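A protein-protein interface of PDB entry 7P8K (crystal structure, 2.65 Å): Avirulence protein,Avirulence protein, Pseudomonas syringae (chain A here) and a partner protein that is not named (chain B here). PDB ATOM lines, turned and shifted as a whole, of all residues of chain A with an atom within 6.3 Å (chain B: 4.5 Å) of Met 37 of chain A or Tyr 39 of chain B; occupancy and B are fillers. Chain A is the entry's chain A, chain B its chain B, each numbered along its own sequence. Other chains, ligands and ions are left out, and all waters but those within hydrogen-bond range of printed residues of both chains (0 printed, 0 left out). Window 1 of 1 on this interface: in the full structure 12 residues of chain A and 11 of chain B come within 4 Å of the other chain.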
ATOM      1  N   GLU A  32      25.732   4.049  30.418  1.00  0.00           N
ATOM      2  CA  GLU A  32      26.865   4.701  29.707  1.00  0.00           C
ATOM      3  C   GLU A  32      26.903   4.247  28.246  1.00  0.00           C
ATOM      4  O   GLU A  32      27.209   5.098  27.376  1.00  0.00           O
ATOM      5  CB  GLU A  32      28.195   4.373  30.377  1.00  0.00           C
ATOM      6  CG  GLU A  32      28.435   5.148  31.655  1.00  0.00           C
ATOM      7  CD  GLU A  32      29.852   5.006  32.176  1.00  0.00           C
ATOM      8  OE1 GLU A  32      30.007   4.645  33.371  1.00  0.00           O
ATOM      9  OE2 GLU A  32      30.799   5.247  31.382  1.00  0.00           O
ATOM     10  N   ASP A  33      26.629   2.962  27.995  1.00  0.00           N
ATOM     11  CA  ASP A  33      26.525   2.378  26.630  1.00  0.00           C
ATOM     12  C   ASP A  33      25.445   3.143  25.855  1.00  0.00           C
ATOM     13  O   ASP A  33      25.680   3.482  24.682  1.00  0.00           O
ATOM     14  CB  ASP A  33      26.209   0.879  26.678  1.00  0.00           C
ATOM     15  CG  ASP A  33      27.390  -0.017  27.008  1.00  0.00           C
ATOM     16  OD1 ASP A  33      28.519   0.309  26.579  1.00  0.00           O
ATOM     17  OD2 ASP A  33      27.170  -1.048  27.691  1.00  0.00           O
ATOM     18  N   LYS A  34      24.304   3.403  26.493  1.00  0.00           N
ATOM     19  CA  LYS A  34      23.165   4.129  25.883  1.00  0.00           C
ATOM     20  C   LYS A  34      23.576   5.587  25.663  1.00  0.00           C
ATOM     21  O   LYS A  34      23.434   6.075  24.523  1.00  0.00           O
ATOM     22  CB  LYS A  34      21.927   4.047  26.778  1.00  0.00           C
ATOM     23  CG  LYS A  34      20.637   4.549  26.133  1.00  0.00           C
ATOM     24  CD  LYS A  34      20.276   3.844  24.832  1.00  0.00           C
ATOM     25  CE  LYS A  34      20.193   2.338  24.976  1.00  0.00           C
ATOM     26  NZ  LYS A  34      19.418   1.733  23.871  1.00  0.00           N
ATOM     27  N   GLN A  35      24.093   6.235  26.712  1.00  0.00           N
ATOM     28  CA  GLN A  35      24.628   7.620  26.650  1.00  0.00           C
ATOM     29  C   GLN A  35      25.635   7.710  25.498  1.00  0.00           C
ATOM     30  O   GLN A  35      25.668   8.764  24.838  1.00  0.00           O
ATOM     31  CB  GLN A  35      25.242   8.035  27.990  1.00  0.00           C
ATOM     32  CG  GLN A  35      25.758   9.467  28.033  1.00  0.00           C
ATOM     33  CD  GLN A  35      24.681  10.520  27.911  1.00  0.00           C
ATOM     34  OE1 GLN A  35      24.197  11.065  28.902  1.00  0.00           O
ATOM     35  NE2 GLN A  35      24.304  10.831  26.682  1.00  0.00           N
ATOM     36  N   LEU A  36      26.403   6.649  25.237  1.00  0.00           N
ATOM     37  CA  LEU A  36      27.395   6.644  24.129  1.00  0.00           C
ATOM     38  C   LEU A  36      26.649   6.703  22.793  1.00  0.00           C
ATOM     39  O   LEU A  36      27.023   7.530  21.941  1.00  0.00           O
ATOM     40  CB  LEU A  36      28.273   5.398  24.228  1.00  0.00           C
ATOM     41  CG  LEU A  36      29.429   5.323  23.233  1.00  0.00           C
ATOM     42  CD1 LEU A  36      30.246   6.606  23.221  1.00  0.00           C
ATOM     43  CD2 LEU A  36      30.322   4.135  23.547  1.00  0.00           C
ATOM     44  N   MET A  37      25.630   5.863  22.622  1.00  0.00           N
ATOM     45  CA  MET A  37      24.823   5.804  21.376  1.00  0.00           C
ATOM     46  C   MET A  37      24.153   7.166  21.182  1.00  0.00           C
ATOM     47  O   MET A  37      24.202   7.696  20.060  1.00  0.00           O
ATOM     48  CB  MET A  37      23.759   4.699  21.441  1.00  0.00           C
ATOM     49  CG  MET A  37      23.099   4.388  20.104  1.00  0.00           C
ATOM     50  SD  MET A  37      24.256   3.800  18.831  1.00  0.00           S
ATOM     51  CE  MET A  37      23.364   4.293  17.357  1.00  0.00           C
ATOM     52  N   VAL A  38      23.589   7.726  22.253  1.00  0.00           N
ATOM     53  CA  VAL A  38      22.960   9.079  22.227  1.00  0.00           C
ATOM     54  C   VAL A  38      23.984  10.087  21.700  1.00  0.00           C
ATOM     55  O   VAL A  38      23.566  11.013  20.984  1.00  0.00           O
ATOM     56  CB  VAL A  38      22.427   9.513  23.604  1.00  0.00           C
ATOM     57  CG1 VAL A  38      21.917  10.946  23.560  1.00  0.00           C
ATOM     58  CG2 VAL A  38      21.344   8.575  24.116  1.00  0.00           C
ATOM     59  N   ASN A  39      25.260   9.921  22.060  1.00  0.00           N
ATOM     60  CA  ASN A  39      26.339  10.860  21.666  1.00  0.00           C
ATOM     61  C   ASN A  39      26.637  10.681  20.179  1.00  0.00           C
ATOM     62  O   ASN A  39      26.813  11.699  19.490  1.00  0.00           O
ATOM     63  CB  ASN A  39      27.590  10.679  22.518  1.00  0.00           C
ATOM     64  CG  ASN A  39      27.378  11.135  23.944  1.00  0.00           C
ATOM     65  OD1 ASN A  39      26.381  11.787  24.251  1.00  0.00           O
ATOM     66  ND2 ASN A  39      28.300  10.783  24.824  1.00  0.00           N
ATOM     67  N   ASN A  40      26.689   9.439  19.702  1.00  0.00           N
ATOM     68  CA  ASN A  40      26.899   9.143  18.262  1.00  0.00           C
ATOM     69  C   ASN A  40      25.767   9.792  17.468  1.00  0.00           C
ATOM     70  O   ASN A  40      26.051  10.525  16.495  1.00  0.00           O
ATOM     71  CB  ASN A  40      26.932   7.643  17.988  1.00  0.00           C
ATOM     72  CG  ASN A  40      28.079   6.962  18.691  1.00  0.00           C
ATOM     73  OD1 ASN A  40      29.230   7.285  18.445  1.00  0.00           O
ATOM     74  ND2 ASN A  40      27.772   6.030  19.571  1.00  0.00           N
ATOM     75  N   LEU A  41      24.530   9.534  17.889  1.00  0.00           N
ATOM     76  CA  LEU A  41      23.318   9.989  17.167  1.00  0.00           C
ATOM     77  C   LEU A  41      23.293  11.514  17.157  1.00  0.00           C
ATOM     78  O   LEU A  41      22.955  12.084  16.104  1.00  0.00           O
ATOM     79  CB  LEU A  41      22.082   9.382  17.826  1.00  0.00           C
ATOM     80  CG  LEU A  41      21.891   7.894  17.537  1.00  0.00           C
ATOM     81  CD1 LEU A  41      20.630   7.360  18.193  1.00  0.00           C
ATOM     82  CD2 LEU A  41      21.867   7.626  16.035  1.00  0.00           C
ATOM     83  N   THR A  42      23.714  12.139  18.258  1.00  0.00           N
ATOM     84  CA  THR A  42      23.841  13.613  18.363  1.00  0.00           C
ATOM     85  C   THR A  42      24.933  14.075  17.392  1.00  0.00           C
ATOM     86  O   THR A  42      24.618  14.927  16.550  1.00  0.00           O
ATOM     87  CB  THR A  42      24.035  14.049  19.818  1.00  0.00           C
ATOM     88  OG1 THR A  42      22.866  13.640  20.525  1.00  0.00           O
ATOM     89  CG2 THR A  42      24.218  15.542  19.962  1.00  0.00           C
ATOM     90  N   GLU A  44      25.949  12.710  14.695  1.00  0.00           N
ATOM     91  CA  GLU A  44      25.459  12.488  13.307  1.00  0.00           C
ATOM     92  C   GLU A  44      24.418  13.574  12.999  1.00  0.00           C
ATOM     93  O   GLU A  44      24.549  14.243  11.955  1.00  0.00           O
ATOM     94  CB  GLU A  44      24.936  11.058  13.133  1.00  0.00           C
ATOM     95  CG  GLU A  44      26.037  10.000  13.075  1.00  0.00           C
ATOM     96  CD  GLU A  44      25.661   8.589  13.527  1.00  0.00           C
ATOM     97  OE1 GLU A  44      24.489   8.376  13.896  1.00  0.00           O
ATOM     98  OE2 GLU A  44      26.554   7.696  13.523  1.00  0.00           O
ATOM     99  N   LEU A  64      17.160   9.341  17.597  1.00  0.00           N
ATOM    100  CA  LEU A  64      17.773   9.991  18.784  1.00  0.00           C
ATOM    101  C   LEU A  64      16.712  10.135  19.883  1.00  0.00           C
ATOM    102  O   LEU A  64      17.068   9.955  21.056  1.00  0.00           O
ATOM    103  CB  LEU A  64      18.364  11.341  18.366  1.00  0.00           C
ATOM    104  CG  LEU A  64      18.995  12.187  19.475  1.00  0.00           C
ATOM    105  CD1 LEU A  64      20.079  11.420  20.218  1.00  0.00           C
ATOM    106  CD2 LEU A  64      19.558  13.479  18.903  1.00  0.00           C
ATOM    107  N   ALA A  67      16.469   6.530  21.467  1.00  0.00           N
ATOM    108  CA  ALA A  67      17.713   6.299  22.237  1.00  0.00           C
ATOM    109  C   ALA A  67      17.680   7.092  23.554  1.00  0.00           C
ATOM    110  O   ALA A  67      18.089   6.535  24.584  1.00  0.00           O
ATOM    111  CB  ALA A  67      18.906   6.669  21.391  1.00  0.00           C
ATOM    112  N   LYS B  24      28.001  -4.997  21.390  1.00  0.00           N
ATOM    113  CA  LYS B  24      27.132  -4.090  20.599  1.00  0.00           C
ATOM    114  C   LYS B  24      26.326  -3.216  21.560  1.00  0.00           C
ATOM    115  O   LYS B  24      25.559  -3.776  22.333  1.00  0.00           O
ATOM    116  CB  LYS B  24      26.181  -4.902  19.714  1.00  0.00           C
ATOM    117  CG  LYS B  24      25.402  -4.091  18.690  1.00  0.00           C
ATOM    118  CD  LYS B  24      24.390  -4.909  17.923  1.00  0.00           C
ATOM    119  CE  LYS B  24      24.119  -4.349  16.543  1.00  0.00           C
ATOM    120  NZ  LYS B  24      22.814  -4.807  16.010  1.00  0.00           N
ATOM    121  N   TYR B  25      26.490  -1.896  21.499  1.00  0.00           N
ATOM    122  CA  TYR B  25      25.770  -0.942  22.380  1.00  0.00           C
ATOM    123  C   TYR B  25      24.625  -0.265  21.617  1.00  0.00           C
ATOM    124  O   TYR B  25      23.776   0.341  22.292  1.00  0.00           O
ATOM    125  CB  TYR B  25      26.746   0.044  23.029  1.00  0.00           C
ATOM    126  CG  TYR B  25      27.415   1.034  22.112  1.00  0.00           C
ATOM    127  CD1 TYR B  25      28.611   0.740  21.476  1.00  0.00           C
ATOM    128  CD2 TYR B  25      26.876   2.294  21.922  1.00  0.00           C
ATOM    129  CE1 TYR B  25      29.244   1.663  20.659  1.00  0.00           C
ATOM    130  CE2 TYR B  25      27.489   3.222  21.101  1.00  0.00           C
ATOM    131  CZ  TYR B  25      28.681   2.911  20.468  1.00  0.00           C
ATOM    132  OH  TYR B  25      29.287   3.828  19.650  1.00  0.00           O
ATOM    133  N   GLY B  26      24.570  -0.377  20.284  1.00  0.00           N
ATOM    134  CA  GLY B  26      23.435   0.149  19.501  1.00  0.00           C
ATOM    135  C   GLY B  26      23.550  -0.095  18.005  1.00  0.00           C
ATOM    136  O   GLY B  26      24.603  -0.579  17.545  1.00  0.00           O
ATOM    137  N   GLN B  27      22.476   0.226  17.275  1.00  0.00           N
ATOM    138  CA  GLN B  27      22.399   0.172  15.792  1.00  0.00           C
ATOM    139  C   GLN B  27      21.557   1.345  15.269  1.00  0.00           C
ATOM    140  O   GLN B  27      20.641   1.795  15.982  1.00  0.00           O
ATOM    141  CB  GLN B  27      21.763  -1.141  15.343  1.00  0.00           C
ATOM    142  CG  GLN B  27      20.358  -1.342  15.895  1.00  0.00           C
ATOM    143  CD  GLN B  27      19.705  -2.618  15.426  1.00  0.00           C
ATOM    144  OE1 GLN B  27      20.292  -3.423  14.705  1.00  0.00           O
ATOM    145  NE2 GLN B  27      18.464  -2.806  15.839  1.00  0.00           N
ATOM    146  N   LYS B  28      21.836   1.795  14.047  1.00  0.00           N
ATOM    147  CA  LYS B  28      21.082   2.876  13.363  1.00  0.00           C
ATOM    148  C   LYS B  28      20.505   2.333  12.054  1.00  0.00           C
ATOM    149  O   LYS B  28      21.254   1.702  11.301  1.00  0.00           O
ATOM    150  CB  LYS B  28      22.007   4.072  13.093  1.00  0.00           C
ATOM    151  CG  LYS B  28      21.338   5.296  12.482  1.00  0.00           C
ATOM    152  CD  LYS B  28      22.330   6.346  12.039  1.00  0.00           C
ATOM    153  CE  LYS B  28      21.729   7.733  12.020  1.00  0.00           C
ATOM    154  NZ  LYS B  28      22.434   8.616  11.067  1.00  0.00           N
ATOM    155  N   ARG B  37      23.461  -0.153  10.661  1.00  0.00           N
ATOM    156  CA  ARG B  37      24.860  -0.007  11.128  1.00  0.00           C
ATOM    157  C   ARG B  37      24.914  -0.443  12.594  1.00  0.00           C
ATOM    158  O   ARG B  37      24.052   0.004  13.374  1.00  0.00           O
ATOM    159  CB  ARG B  37      25.342   1.435  10.965  1.00  0.00           C
ATOM    160  CG  ARG B  37      26.807   1.650  11.319  1.00  0.00           C
ATOM    161  CD  ARG B  37      27.172   3.122  11.309  1.00  0.00           C
ATOM    162  NE  ARG B  37      26.800   3.744  10.044  1.00  0.00           N
ATOM    163  CZ  ARG B  37      26.328   4.980   9.906  1.00  0.00           C
ATOM    164  NH1 ARG B  37      26.007   5.433   8.706  1.00  0.00           N
ATOM    165  NH2 ARG B  37      26.156   5.754  10.963  1.00  0.00           N
ATOM    166  N   GLY B  38      25.878  -1.303  12.923  1.00  0.00           N
ATOM    167  CA  GLY B  38      26.154  -1.775  14.292  1.00  0.00           C
ATOM    168  C   GLY B  38      27.207  -0.916  14.969  1.00  0.00           C
ATOM    169  O   GLY B  38      28.267  -0.653  14.347  1.00  0.00           O
ATOM    170  N   TYR B  39      26.917  -0.472  16.193  1.00  0.00           N
ATOM    171  CA  TYR B  39      27.834   0.330  17.029  1.00  0.00           C
ATOM    172  C   TYR B  39      28.333  -0.573  18.151  1.00  0.00           C
ATOM    173  O   TYR B  39      27.489  -1.026  18.953  1.00  0.00           O
ATOM    174  CB  TYR B  39      27.131   1.583  17.548  1.00  0.00           C
ATOM    175  CG  TYR B  39      26.709   2.559  16.481  1.00  0.00           C
ATOM    176  CD1 TYR B  39      25.681   2.261  15.602  1.00  0.00           C
ATOM    177  CD2 TYR B  39      27.319   3.801  16.365  1.00  0.00           C
ATOM    178  CE1 TYR B  39      25.277   3.163  14.632  1.00  0.00           C
ATOM    179  CE2 TYR B  39      26.927   4.716  15.400  1.00  0.00           C
ATOM    180  CZ  TYR B  39      25.892   4.401  14.537  1.00  0.00           C
ATOM    181  OH  TYR B  39      25.491   5.297  13.586  1.00  0.00           O
ATOM    182  N   TYR B  40      29.646  -0.829  18.175  1.00  0.00           N
ATOM    183  CA  TYR B  40      30.327  -1.790  19.086  1.00  0.00           C
ATOM    184  C   TYR B  40      31.398  -1.067  19.911  1.00  0.00           C
ATOM    185  O   TYR B  40      32.145  -0.233  19.331  1.00  0.00           O
ATOM    186  CB  TYR B  40      30.971  -2.921  18.280  1.00  0.00           C
ATOM    187  CG  TYR B  40      30.011  -3.773  17.486  1.00  0.00           C
ATOM    188  CD1 TYR B  40      29.587  -3.376  16.228  1.00  0.00           C
ATOM    189  CD2 TYR B  40      29.529  -4.977  17.982  1.00  0.00           C
ATOM    190  CE1 TYR B  40      28.709  -4.146  15.485  1.00  0.00           C
ATOM    191  CE2 TYR B  40      28.657  -5.766  17.246  1.00  0.00           C
ATOM    192  CZ  TYR B  40      28.244  -5.348  15.994  1.00  0.00           C
ATOM    193  OH  TYR B  40      27.379  -6.099  15.251  1.00  0.00           O
ATOM    194  N   ARG B  41      31.475  -1.399  21.208  1.00  0.00           N
ATOM    195  CA  ARG B  41      32.513  -0.919  22.166  1.00  0.00           C
ATOM    196  C   ARG B  41      33.284  -2.116  22.727  1.00  0.00           C
ATOM    197  O   ARG B  41      32.714  -3.209  22.783  1.00  0.00           O
ATOM    198  CB  ARG B  41      31.902  -0.085  23.297  1.00  0.00           C
ATOM    199  CG  ARG B  41      30.748  -0.737  24.043  1.00  0.00           C
ATOM    200  CD  ARG B  41      31.177  -1.707  25.125  1.00  0.00           C
ATOM    201  NE  ARG B  41      30.169  -1.801  26.173  1.00  0.00           N
ATOM    202  CZ  ARG B  41      30.090  -2.771  27.078  1.00  0.00           C
ATOM    203  NH1 ARG B  41      30.965  -3.762  27.087  1.00  0.00           N
ATOM    204  NH2 ARG B  41      29.124  -2.748  27.978  1.00  0.00           N
ATOM    205  N   LYS B  54      33.995   0.487  17.220  1.00  0.00           N
ATOM    206  CA  LYS B  54      33.975   0.227  15.758  1.00  0.00           C
ATOM    207  C   LYS B  54      32.532   0.280  15.271  1.00  0.00           C
ATOM    208  O   LYS B  54      31.628  -0.076  16.041  1.00  0.00           O
ATOM    209  CB  LYS B  54      34.655  -1.106  15.425  1.00  0.00           C
ATOM    210  CG  LYS B  54      33.887  -2.383  15.758  1.00  0.00           C
ATOM    211  CD  LYS B  54      34.429  -3.606  15.021  1.00  0.00           C
ATOM    212  CE  LYS B  54      33.728  -4.899  15.381  1.00  0.00           C
ATOM    213  NZ  LYS B  54      34.354  -6.066  14.714  1.00  0.00           N
ATOM    214  N   GLN B  55      32.338   0.719  14.036  1.00  0.00           N
ATOM    215  CA  GLN B  55      31.012   0.752  13.370  1.00  0.00           C
ATOM    216  C   GLN B  55      31.063  -0.177  12.158  1.00  0.00           C
ATOM    217  O   GLN B  55      32.006  -0.056  11.354  1.00  0.00           O
ATOM    218  CB  GLN B  55      30.649   2.183  12.995  1.00  0.00           C
ATOM    219  CG  GLN B  55      30.315   3.036  14.203  1.00  0.00           C
ATOM    220  CD  GLN B  55      29.983   4.452  13.811  1.00  0.00           C
ATOM    221  OE1 GLN B  55      29.830   4.779  12.637  1.00  0.00           O
ATOM    222  NE2 GLN B  55      29.873   5.314  14.803  1.00  0.00           N
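NZ of Lys 24 of chain B lies within hydrogen-bond range of OE1 of Gln 27 of chain B (3.2 Å). The backbone carbonyl oxygen (O) of Tyr 39 of chain B is in hydrogen-bond range of the backbone NH (N) of Tyr 25 of chain B, at 2.9 Å. The backbone carbonyl oxygen (O) of Gly 26 of chain B sits at hydrogen-bond distance from the backbone NH (N) of Tyr 39 of chain B. The backbone NH of Lys 28 of chain B is in hydrogen-bond range of the backbone carbonyl oxygen of Arg 37 of chain B (2.9 Å). OH of Tyr 39 of chain B lies within hydrogen-bond range of NH2 of Arg 37 of chain B, 2.7 Å away. The side-chain amide nitrogen of Asn 40 of chain A is in hydrogen-bond range of the backbone carbonyl oxygen of Leu 36 of chain A (2.9 Å).
Of the printed residues of chain B, Leu 36 of chain A touches Tyr 25 (3.6 Å). Of chain B, only Tyr 25 (3.6 Å), Gly 26 (3.8 Å), Gln 27 (3.9 Å) and Tyr 39 (3.5 Å) come within 4 Å of Met 37 of chain A. Printed residues of chain A within 4 Å of Gly 26 of chain B: Met 37 (3.8 Å). Printed residues of chain A within 4 Å of Arg 37 of chain B: Glu 44. Of the printed residues of chain A, Tyr 39 of chain B touches Met 37 (3.5 Å), Asn 40 (3.9 Å) and Glu 44 (2.6 Å). The nearest residue of chain B that does not touch Met 37 of chain A is Lys 28 of chain B (4.4 Å). The nearest residue of chain A that does not touch Tyr 39 of chain B is Leu 41 of chain A (5.0 Å).
The side-chain hydroxyl (OH) of Tyr 25 of chain B is in hydrogen-bond range of the side-chain amide nitrogen (ND2) of Asn 40 of chain A. OE1 of Glu 44 of chain A is in salt-bridge range of NZ of Lys 28 of chain B (3.5 Å). NH2 of Arg 37 of chain B lies within salt-bridge range of OE2 of Glu 44 of chain A, 3.2 Å away. OH of Tyr 39 of chain B sits at hydrogen-bond distance from OE2 of Glu 44 of chain A (2.6 Å). The guanidinium group (NH2) of Arg 41 of chain B is in salt-bridge range of the side-chain carboxylate (OD2) of Asp 33 of chain A, at 2.6 Å.
Among the printed residues, pairs that only touch across the chains: Asp 33 of chain A with Tyr 25 of chain B (3.2 Å), Leu 36 of chain A with Tyr 25 of chain B (3.6 Å), Met 37 of chain A with Tyr 25 of chain B (3.6 Å), Met 37 of chain A with Gly 26 of chain B (3.8 Å), Met 37 of chain A with Gln 27 of chain B (3.9 Å), Met 37 of chain A with Tyr 39 of chain B (3.5 Å) and Asn 40 of chain A with Tyr 39 of chain B (3.9 Å).
Of the 14 printed residues of chain A, 5 touch a printed residue of chain B. Hydrophobic or aromatic side chains of chain A within 4 Å of the printed part of chain B: Leu 36 and Met 37. Along chain A the printed residues that touch a printed residue of chain B span positions 33 to 44. Hydrophobic or aromatic side chains of chain B that line the printed part of chain A: Tyr 25 and Tyr 39. Among the printed residues, 12 pairs touch across the chains.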
